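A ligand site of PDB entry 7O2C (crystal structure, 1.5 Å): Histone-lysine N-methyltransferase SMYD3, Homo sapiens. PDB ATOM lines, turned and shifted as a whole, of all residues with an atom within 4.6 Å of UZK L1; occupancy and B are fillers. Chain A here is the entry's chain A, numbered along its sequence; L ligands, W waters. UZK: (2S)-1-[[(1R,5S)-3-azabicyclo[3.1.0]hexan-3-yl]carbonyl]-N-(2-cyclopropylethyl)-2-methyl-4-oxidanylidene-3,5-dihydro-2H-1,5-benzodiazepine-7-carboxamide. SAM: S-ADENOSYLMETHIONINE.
O of Cys 180 touches C20 of UZK L1, at 3.7 Å. Ser 182 touches UZK L1 (O to C18, 3.7 Å). Phe 183 touches UZK L1 (CA to O21, 3.2 Å). O of Ile 214 touches C9 of UZK L1, 3.7 Å away. Phe 216 touches UZK L1 (CD2 to O12, 3.3 Å). Tyr 257 touches UZK L1 (OH to C16, 3.5 Å). CE1 of His 366 touches C13 of UZK L1, at 3.6 Å. Val 368 touches UZK L1 (CG2 to O24, 3.4 Å). Within 4 Å of UZK L1: Cys 180, Ser 182, Phe 183, Thr 184, Cys 186, Ile 214, Phe 216, Tyr 239, Tyr 257, His 366 and Val 368.
The backbone carbonyl oxygen (O) of Tyr 239 is in hydrogen-bond range of a nitrogen (N15) of UZK L1. The side-chain sulfur of Cys 186 sits close to an oxygen (O12) of UZK L1 (3.3 Å). The backbone carbonyl oxygen of Tyr 257 lies within hydrogen-bond range of an oxygen (O3') of SAM L2 (2.6 Å). An oxygen (O12) of UZK L1 lies close to the backbone NH of Cys 186 (3.4 Å). The backbone NH of Thr 184 is in hydrogen-bond range of an oxygen (O21) of UZK L1, 2.9 Å away. A nitrogen (N11) of UZK L1 sits at hydrogen-bond distance from the backbone carbonyl oxygen of Thr 184, 2.8 Å away.
Water W1 lies within hydrogen-bond range of an oxygen (O12) of UZK L1, the backbone NH (N) of Phe 216 and the side-chain sulfur (SD) of Met 190.
The side-chain sulfur (SG) of Cys 180 lies within hydrogen-bond range of the side-chain amide nitrogen (ND2) of Asn 181. A ring nitrogen (ND1) of His 366 is in hydrogen-bond range of the backbone NH (N) of Val 368 (3.0 Å).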
ATOM      1  N   CYS A 180       4.618  13.403  -9.382  1.00  0.00           N
ATOM      2  CA  CYS A 180       4.356  14.837  -9.272  1.00  0.00           C
ATOM      3  C   CYS A 180       5.503  15.573  -8.537  1.00  0.00           C
ATOM      4  O   CYS A 180       5.340  16.768  -8.377  1.00  0.00           O
ATOM      5  CB  CYS A 180       3.007  15.201  -8.687  1.00  0.00           C
ATOM      6  SG  CYS A 180       2.863  14.760  -6.944  1.00  0.00           S
ATOM      7  N   ASN A 181       6.612  14.905  -8.226  1.00  0.00           N
ATOM      8  CA  ASN A 181       7.805  15.517  -7.592  1.00  0.00           C
ATOM      9  C   ASN A 181       9.134  15.231  -8.320  1.00  0.00           C
ATOM     10  O   ASN A 181      10.126  15.705  -7.842  1.00  0.00           O
ATOM     11  CB  ASN A 181       7.885  15.174  -6.134  1.00  0.00           C
ATOM     12  CG  ASN A 181       6.674  15.716  -5.362  1.00  0.00           C
ATOM     13  OD1 ASN A 181       6.645  16.889  -5.005  1.00  0.00           O
ATOM     14  ND2 ASN A 181       5.705  14.847  -5.035  1.00  0.00           N
ATOM     15  N   SER A 182       9.131  14.519  -9.428  1.00  0.00           N
ATOM     16  CA  SER A 182      10.367  14.192 -10.165  1.00  0.00           C
ATOM     17  C   SER A 182      10.882  15.475 -10.841  1.00  0.00           C
ATOM     18  O   SER A 182      10.150  16.095 -11.513  1.00  0.00           O
ATOM     19  CB  SER A 182      10.138  13.168 -11.245  1.00  0.00           C
ATOM     20  OG  SER A 182      10.059  11.906 -10.667  1.00  0.00           O
ATOM     21  N   PHE A 183      12.162  15.748 -10.665  1.00  0.00           N
ATOM     22  CA  PHE A 183      12.864  16.824 -11.414  1.00  0.00           C
ATOM     23  C   PHE A 183      13.589  16.219 -12.608  1.00  0.00           C
ATOM     24  O   PHE A 183      14.326  15.267 -12.496  1.00  0.00           O
ATOM     25  CB  PHE A 183      13.818  17.537 -10.493  1.00  0.00           C
ATOM     26  CG  PHE A 183      13.138  18.465  -9.519  1.00  0.00           C
ATOM     27  CD1 PHE A 183      12.920  19.808  -9.752  1.00  0.00           C
ATOM     28  CD2 PHE A 183      12.654  17.924  -8.331  1.00  0.00           C
ATOM     29  CE1 PHE A 183      12.276  20.604  -8.823  1.00  0.00           C
ATOM     30  CE2 PHE A 183      12.013  18.733  -7.385  1.00  0.00           C
ATOM     31  CZ  PHE A 183      11.775  20.063  -7.638  1.00  0.00           C
ATOM     32  N   THR A 184      13.428  16.910 -13.730  1.00  0.00           N
ATOM     33  CA  THR A 184      14.211  16.558 -14.943  1.00  0.00           C
ATOM     34  C   THR A 184      15.577  17.255 -14.890  1.00  0.00           C
ATOM     35  O   THR A 184      15.622  18.510 -14.957  1.00  0.00           O
ATOM     36  CB  THR A 184      13.435  16.983 -16.182  1.00  0.00           C
ATOM     37  OG1 THR A 184      12.123  16.385 -16.202  1.00  0.00           O
ATOM     38  CG2 THR A 184      14.148  16.621 -17.461  1.00  0.00           C
ATOM     39  N   ILE A 185      16.645  16.485 -14.932  1.00  0.00           N
ATOM     40  CA  ILE A 185      18.036  17.012 -14.801  1.00  0.00           C
ATOM     41  C   ILE A 185      18.537  17.192 -16.231  1.00  0.00           C
ATOM     42  O   ILE A 185      18.574  16.226 -17.032  1.00  0.00           O
ATOM     43  CB  ILE A 185      18.932  16.061 -13.988  1.00  0.00           C
ATOM     44  CG1 ILE A 185      18.383  15.798 -12.589  1.00  0.00           C
ATOM     45  CG2 ILE A 185      20.357  16.617 -13.977  1.00  0.00           C
ATOM     46  CD1 ILE A 185      19.014  14.634 -11.876  1.00  0.00           C
ATOM     47  N   CYS A 186      18.834  18.442 -16.588  1.00  0.00           N
ATOM     48  CA  CYS A 186      19.505  18.703 -17.884  1.00  0.00           C
ATOM     49  C   CYS A 186      20.969  19.022 -17.687  1.00  0.00           C
ATOM     50  O   CYS A 186      21.389  19.481 -16.626  1.00  0.00           O
ATOM     51  CB  CYS A 186      18.853  19.886 -18.546  1.00  0.00           C
ATOM     52  SG  CYS A 186      17.125  19.633 -18.992  1.00  0.00           S
ATOM     53  N   MET A 190      21.636  21.985 -21.759  1.00  0.00           N
ATOM     54  CA  MET A 190      20.160  21.952 -21.587  1.00  0.00           C
ATOM     55  C   MET A 190      19.504  20.690 -22.211  1.00  0.00           C
ATOM     56  O   MET A 190      18.321  20.714 -22.545  1.00  0.00           O
ATOM     57  CB  MET A 190      19.476  23.203 -22.069  1.00  0.00           C
ATOM     58  CG  MET A 190      19.616  24.337 -21.038  1.00  0.00           C
ATOM     59  SD  MET A 190      18.797  23.897 -19.457  1.00  0.00           S
ATOM     60  CE  MET A 190      19.399  25.359 -18.626  1.00  0.00           C
ATOM     61  N   GLU A 192      18.199  16.981 -21.634  1.00  0.00           N
ATOM     62  CA  GLU A 192      17.770  16.041 -20.577  1.00  0.00           C
ATOM     63  C   GLU A 192      18.777  14.875 -20.473  1.00  0.00           C
ATOM     64  O   GLU A 192      19.025  14.178 -21.444  1.00  0.00           O
ATOM     65  CB  GLU A 192      16.351  15.574 -20.900  1.00  0.00           C
ATOM     66  CG  GLU A 192      15.881  14.486 -19.949  1.00  0.00           C
ATOM     67  CD  GLU A 192      14.436  14.096 -20.191  1.00  0.00           C
ATOM     68  OE1 GLU A 192      13.809  14.762 -21.047  1.00  0.00           O
ATOM     69  OE2 GLU A 192      13.961  13.125 -19.520  1.00  0.00           O
ATOM     70  N   ILE A 214      15.180  27.039 -11.662  1.00  0.00           N
ATOM     71  CA  ILE A 214      16.149  26.022 -11.284  1.00  0.00           C
ATOM     72  C   ILE A 214      17.104  25.767 -12.463  1.00  0.00           C
ATOM     73  O   ILE A 214      16.727  25.824 -13.632  1.00  0.00           O
ATOM     74  CB  ILE A 214      15.471  24.740 -10.806  1.00  0.00           C
ATOM     75  CG1 ILE A 214      14.598  24.153 -11.902  1.00  0.00           C
ATOM     76  CG2 ILE A 214      14.751  25.010  -9.494  1.00  0.00           C
ATOM     77  CD1 ILE A 214      14.043  22.792 -11.554  1.00  0.00           C
ATOM     78  N   PHE A 216      20.732  23.019 -13.200  1.00  0.00           N
ATOM     79  CA  PHE A 216      21.500  21.854 -12.754  1.00  0.00           C
ATOM     80  C   PHE A 216      22.934  22.029 -13.229  1.00  0.00           C
ATOM     81  O   PHE A 216      23.186  22.415 -14.414  1.00  0.00           O
ATOM     82  CB  PHE A 216      20.940  20.534 -13.267  1.00  0.00           C
ATOM     83  CG  PHE A 216      19.553  20.293 -12.736  1.00  0.00           C
ATOM     84  CD1 PHE A 216      19.405  19.502 -11.601  1.00  0.00           C
ATOM     85  CD2 PHE A 216      18.437  20.820 -13.371  1.00  0.00           C
ATOM     86  CE1 PHE A 216      18.120  19.310 -11.078  1.00  0.00           C
ATOM     87  CE2 PHE A 216      17.176  20.596 -12.850  1.00  0.00           C
ATOM     88  CZ  PHE A 216      17.040  19.862 -11.681  1.00  0.00           C
ATOM     89  N   ILE A 237       8.246  28.174  -9.623  1.00  0.00           N
ATOM     90  CA  ILE A 237       8.987  27.854 -10.860  1.00  0.00           C
ATOM     91  C   ILE A 237       8.005  27.396 -11.895  1.00  0.00           C
ATOM     92  O   ILE A 237       6.857  27.014 -11.555  1.00  0.00           O
ATOM     93  CB  ILE A 237      10.032  26.774 -10.639  1.00  0.00           C
ATOM     94  CG1 ILE A 237       9.403  25.498 -10.072  1.00  0.00           C
ATOM     95  CG2 ILE A 237      11.147  27.333  -9.773  1.00  0.00           C
ATOM     96  CD1 ILE A 237      10.324  24.300 -10.077  1.00  0.00           C
ATOM     97  N   CYS A 238       8.395  27.416 -13.147  1.00  0.00           N
ATOM     98  CA  CYS A 238       7.559  26.830 -14.191  1.00  0.00           C
ATOM     99  C   CYS A 238       7.906  25.346 -14.316  1.00  0.00           C
ATOM    100  O   CYS A 238       9.088  24.960 -14.541  1.00  0.00           O
ATOM    101  CB  CYS A 238       7.725  27.554 -15.524  1.00  0.00           C
ATOM    102  SG  CYS A 238       6.547  26.913 -16.751  1.00  0.00           S
ATOM    103  N   TYR A 239       6.950  24.451 -14.057  1.00  0.00           N
ATOM    104  CA  TYR A 239       7.262  23.002 -14.117  1.00  0.00           C
ATOM    105  C   TYR A 239       7.535  22.538 -15.561  1.00  0.00           C
ATOM    106  O   TYR A 239       8.052  21.425 -15.729  1.00  0.00           O
ATOM    107  CB  TYR A 239       6.113  22.154 -13.543  1.00  0.00           C
ATOM    108  CG  TYR A 239       5.814  22.265 -12.077  1.00  0.00           C
ATOM    109  CD1 TYR A 239       6.567  23.008 -11.182  1.00  0.00           C
ATOM    110  CD2 TYR A 239       4.759  21.549 -11.558  1.00  0.00           C
ATOM    111  CE1 TYR A 239       6.330  23.081  -9.827  1.00  0.00           C
ATOM    112  CE2 TYR A 239       4.496  21.617 -10.224  1.00  0.00           C
ATOM    113  CZ  TYR A 239       5.257  22.340  -9.338  1.00  0.00           C
ATOM    114  OH  TYR A 239       4.942  22.372  -8.012  1.00  0.00           O
ATOM    115  N   ASP A 241       8.269  22.936 -19.930  1.00  0.00           N
ATOM    116  CA  ASP A 241       8.718  23.529 -21.211  1.00  0.00           C
ATOM    117  C   ASP A 241       7.935  24.800 -21.473  1.00  0.00           C
ATOM    118  O   ASP A 241       6.736  24.775 -21.468  1.00  0.00           O
ATOM    119  CB  ASP A 241       8.539  22.467 -22.280  1.00  0.00           C
ATOM    120  CG  ASP A 241       8.749  22.846 -23.744  1.00  0.00           C
ATOM    121  OD1 ASP A 241       9.408  23.886 -24.040  1.00  0.00           O
ATOM    122  OD2 ASP A 241       8.197  22.051 -24.619  1.00  0.00           O
ATOM    123  N   TYR A 257       0.116  16.485 -12.602  1.00  0.00           N
ATOM    124  CA  TYR A 257       0.143  17.270 -11.331  1.00  0.00           C
ATOM    125  C   TYR A 257      -1.212  17.403 -10.635  1.00  0.00           C
ATOM    126  O   TYR A 257      -1.237  17.973  -9.571  1.00  0.00           O
ATOM    127  CB  TYR A 257       0.818  18.629 -11.599  1.00  0.00           C
ATOM    128  CG  TYR A 257       2.260  18.438 -12.042  1.00  0.00           C
ATOM    129  CD1 TYR A 257       3.253  18.144 -11.141  1.00  0.00           C
ATOM    130  CD2 TYR A 257       2.621  18.611 -13.352  1.00  0.00           C
ATOM    131  CE1 TYR A 257       4.570  17.971 -11.480  1.00  0.00           C
ATOM    132  CE2 TYR A 257       3.977  18.504 -13.709  1.00  0.00           C
ATOM    133  CZ  TYR A 257       4.945  18.155 -12.800  1.00  0.00           C
ATOM    134  OH  TYR A 257       6.270  17.961 -13.090  1.00  0.00           O
ATOM    135  N   HIS A 366      15.567  33.617 -18.198  1.00  0.00           N
ATOM    136  CA  HIS A 366      15.286  32.170 -18.193  1.00  0.00           C
ATOM    137  C   HIS A 366      16.541  31.425 -18.642  1.00  0.00           C
ATOM    138  O   HIS A 366      17.135  31.756 -19.678  1.00  0.00           O
ATOM    139  CB  HIS A 366      14.139  31.887 -19.156  1.00  0.00           C
ATOM    140  CG  HIS A 366      13.601  30.509 -19.056  1.00  0.00           C
ATOM    141  ND1 HIS A 366      14.337  29.386 -19.330  1.00  0.00           N
ATOM    142  CD2 HIS A 366      12.329  30.114 -18.777  1.00  0.00           C
ATOM    143  CE1 HIS A 366      13.538  28.262 -19.169  1.00  0.00           C
ATOM    144  NE2 HIS A 366      12.294  28.733 -18.766  1.00  0.00           N
ATOM    145  N   PRO A 367      16.958  30.356 -17.945  1.00  0.00           N
ATOM    146  CA  PRO A 367      18.263  29.740 -18.216  1.00  0.00           C
ATOM    147  C   PRO A 367      18.281  29.203 -19.648  1.00  0.00           C
ATOM    148  O   PRO A 367      19.345  29.040 -20.178  1.00  0.00           O
ATOM    149  CB  PRO A 367      18.389  28.631 -17.151  1.00  0.00           C
ATOM    150  CG  PRO A 367      16.931  28.381 -16.743  1.00  0.00           C
ATOM    151  CD  PRO A 367      16.288  29.756 -16.773  1.00  0.00           C
ATOM    152  N   VAL A 368      17.172  28.722 -20.193  1.00  0.00           N
ATOM    153  CA  VAL A 368      17.191  28.109 -21.542  1.00  0.00           C
ATOM    154  C   VAL A 368      17.562  29.178 -22.565  1.00  0.00           C
ATOM    155  O   VAL A 368      18.303  28.835 -23.515  1.00  0.00           O
ATOM    156  CB  VAL A 368      15.829  27.436 -21.839  1.00  0.00           C
ATOM    157  CG1 VAL A 368      15.647  27.088 -23.289  1.00  0.00           C
ATOM    158  CG2 VAL A 368      15.703  26.241 -21.003  1.00  0.00           C
HETATM  159  C4  UZK L   1      13.546  21.997 -16.955  1.00  0.00           C
HETATM  160  C5  UZK L   1      12.100  22.227 -16.966  1.00  0.00           C
HETATM  161  C6  UZK L   1      11.401  21.561 -15.920  1.00  0.00           C
HETATM  162  C8  UZK L   1      15.084  23.797 -17.672  1.00  0.00           C
HETATM  163  C10 UZK L   1      16.390  22.036 -16.360  1.00  0.00           C
HETATM  164  C13 UZK L   1      14.353  25.079 -17.580  1.00  0.00           C
HETATM  165  C17 UZK L   1       9.467  20.304 -11.310  1.00  0.00           C
HETATM  166  C20 UZK L   1       7.591  19.366  -9.793  1.00  0.00           C
HETATM  167  C22 UZK L   1      13.818  22.454 -19.292  1.00  0.00           C
HETATM  168  C26 UZK L   1      13.128  19.824 -21.507  1.00  0.00           C
HETATM  169  C28 UZK L   1      13.091  20.136 -19.060  1.00  0.00           C
HETATM  170  C25 UZK L   1      12.690  21.181 -21.085  1.00  0.00           C
HETATM  171  C29 UZK L   1      14.622  19.559 -21.310  1.00  0.00           C
HETATM  172  C27 UZK L   1      13.600  19.138 -20.158  1.00  0.00           C
HETATM  173  N23 UZK L   1      13.095  21.384 -19.735  1.00  0.00           N
HETATM  174  O24 UZK L   1      14.103  23.309 -20.179  1.00  0.00           O
HETATM  175  N7  UZK L   1      14.170  22.648 -18.040  1.00  0.00           N
HETATM  176  C9  UZK L   1      15.867  23.448 -16.368  1.00  0.00           C
HETATM  177  O12 UZK L   1      17.544  21.636 -16.403  1.00  0.00           O
HETATM  178  N11 UZK L   1      15.517  21.075 -16.017  1.00  0.00           N
HETATM  179  C3  UZK L   1      14.143  21.259 -16.037  1.00  0.00           C
HETATM  180  C2  UZK L   1      13.426  20.628 -14.959  1.00  0.00           C
HETATM  181  C1  UZK L   1      12.015  20.772 -14.971  1.00  0.00           C
HETATM  182  C14 UZK L   1      11.237  20.047 -13.855  1.00  0.00           C
HETATM  183  O21 UZK L   1      11.881  19.300 -13.156  1.00  0.00           O
HETATM  184  N15 UZK L   1       9.917  20.290 -13.782  1.00  0.00           N
HETATM  185  C16 UZK L   1       9.269  19.620 -12.632  1.00  0.00           C
HETATM  186  C18 UZK L   1       9.070  19.322 -10.174  1.00  0.00           C
HETATM  187  C19 UZK L   1       8.685  20.020  -8.901  1.00  0.00           C
HETATM  188  N   SAM L   2       2.042  21.935  -3.077  1.00  0.00           N
HETATM  189  CA  SAM L   2       3.034  20.822  -3.017  1.00  0.00           C
HETATM  190  C   SAM L   2       3.078  20.185  -1.609  1.00  0.00           C
HETATM  191  O   SAM L   2       3.936  19.388  -1.374  1.00  0.00           O
HETATM  192  OXT SAM L   2       2.131  20.498  -0.849  1.00  0.00           O
HETATM  193  CB  SAM L   2       4.428  21.311  -3.447  1.00  0.00           C
HETATM  194  CG  SAM L   2       4.604  21.286  -4.972  1.00  0.00           C
HETATM  195  SD  SAM L   2       4.670  19.607  -5.591  1.00  0.00           S
HETATM  196  CE  SAM L   2       6.126  19.509  -6.584  1.00  0.00           C
HETATM  197  C5' SAM L   2       3.481  19.592  -6.946  1.00  0.00           C
HETATM  198  C4' SAM L   2       2.005  19.625  -6.552  1.00  0.00           C
HETATM  199  O4' SAM L   2       1.700  20.872  -5.906  1.00  0.00           O
HETATM  200  C3' SAM L   2       1.002  19.513  -7.678  1.00  0.00           C
HETATM  201  O3' SAM L   2       0.873  18.166  -8.108  1.00  0.00           O
HETATM  202  C2' SAM L   2      -0.245  20.169  -7.053  1.00  0.00           C
HETATM  203  O2' SAM L   2      -0.799  19.302  -6.073  1.00  0.00           O
HETATM  204  C1' SAM L   2       0.408  21.325  -6.288  1.00  0.00           C
HETATM  205  N9  SAM L   2       0.559  22.536  -7.094  1.00  0.00           N
HETATM  206  C8  SAM L   2       1.711  23.042  -7.675  1.00  0.00           C
HETATM  207  N7  SAM L   2       1.515  24.170  -8.328  1.00  0.00           N
HETATM  208  C5  SAM L   2       0.177  24.447  -8.187  1.00  0.00           C
HETATM  209  C6  SAM L   2      -0.611  25.500  -8.656  1.00  0.00           C
HETATM  210  N6  SAM L   2      -0.123  26.554  -9.325  1.00  0.00           N
HETATM  211  N1  SAM L   2      -1.936  25.485  -8.380  1.00  0.00           N
HETATM  212  C2  SAM L   2      -2.397  24.424  -7.664  1.00  0.00           C
HETATM  213  N3  SAM L   2      -1.735  23.390  -7.149  1.00  0.00           N
HETATM  214  C4  SAM L   2      -0.413  23.439  -7.434  1.00  0.00           C
HETATM  215  O   HOH W   1      19.652  23.368 -15.916  1.00  0.00           O
HETATM  216  O   HOH W   2      12.128  25.163 -20.753  1.00  0.00           O
HETATM  217  O   HOH W   3      15.448  22.828 -22.600  1.00  0.00           O
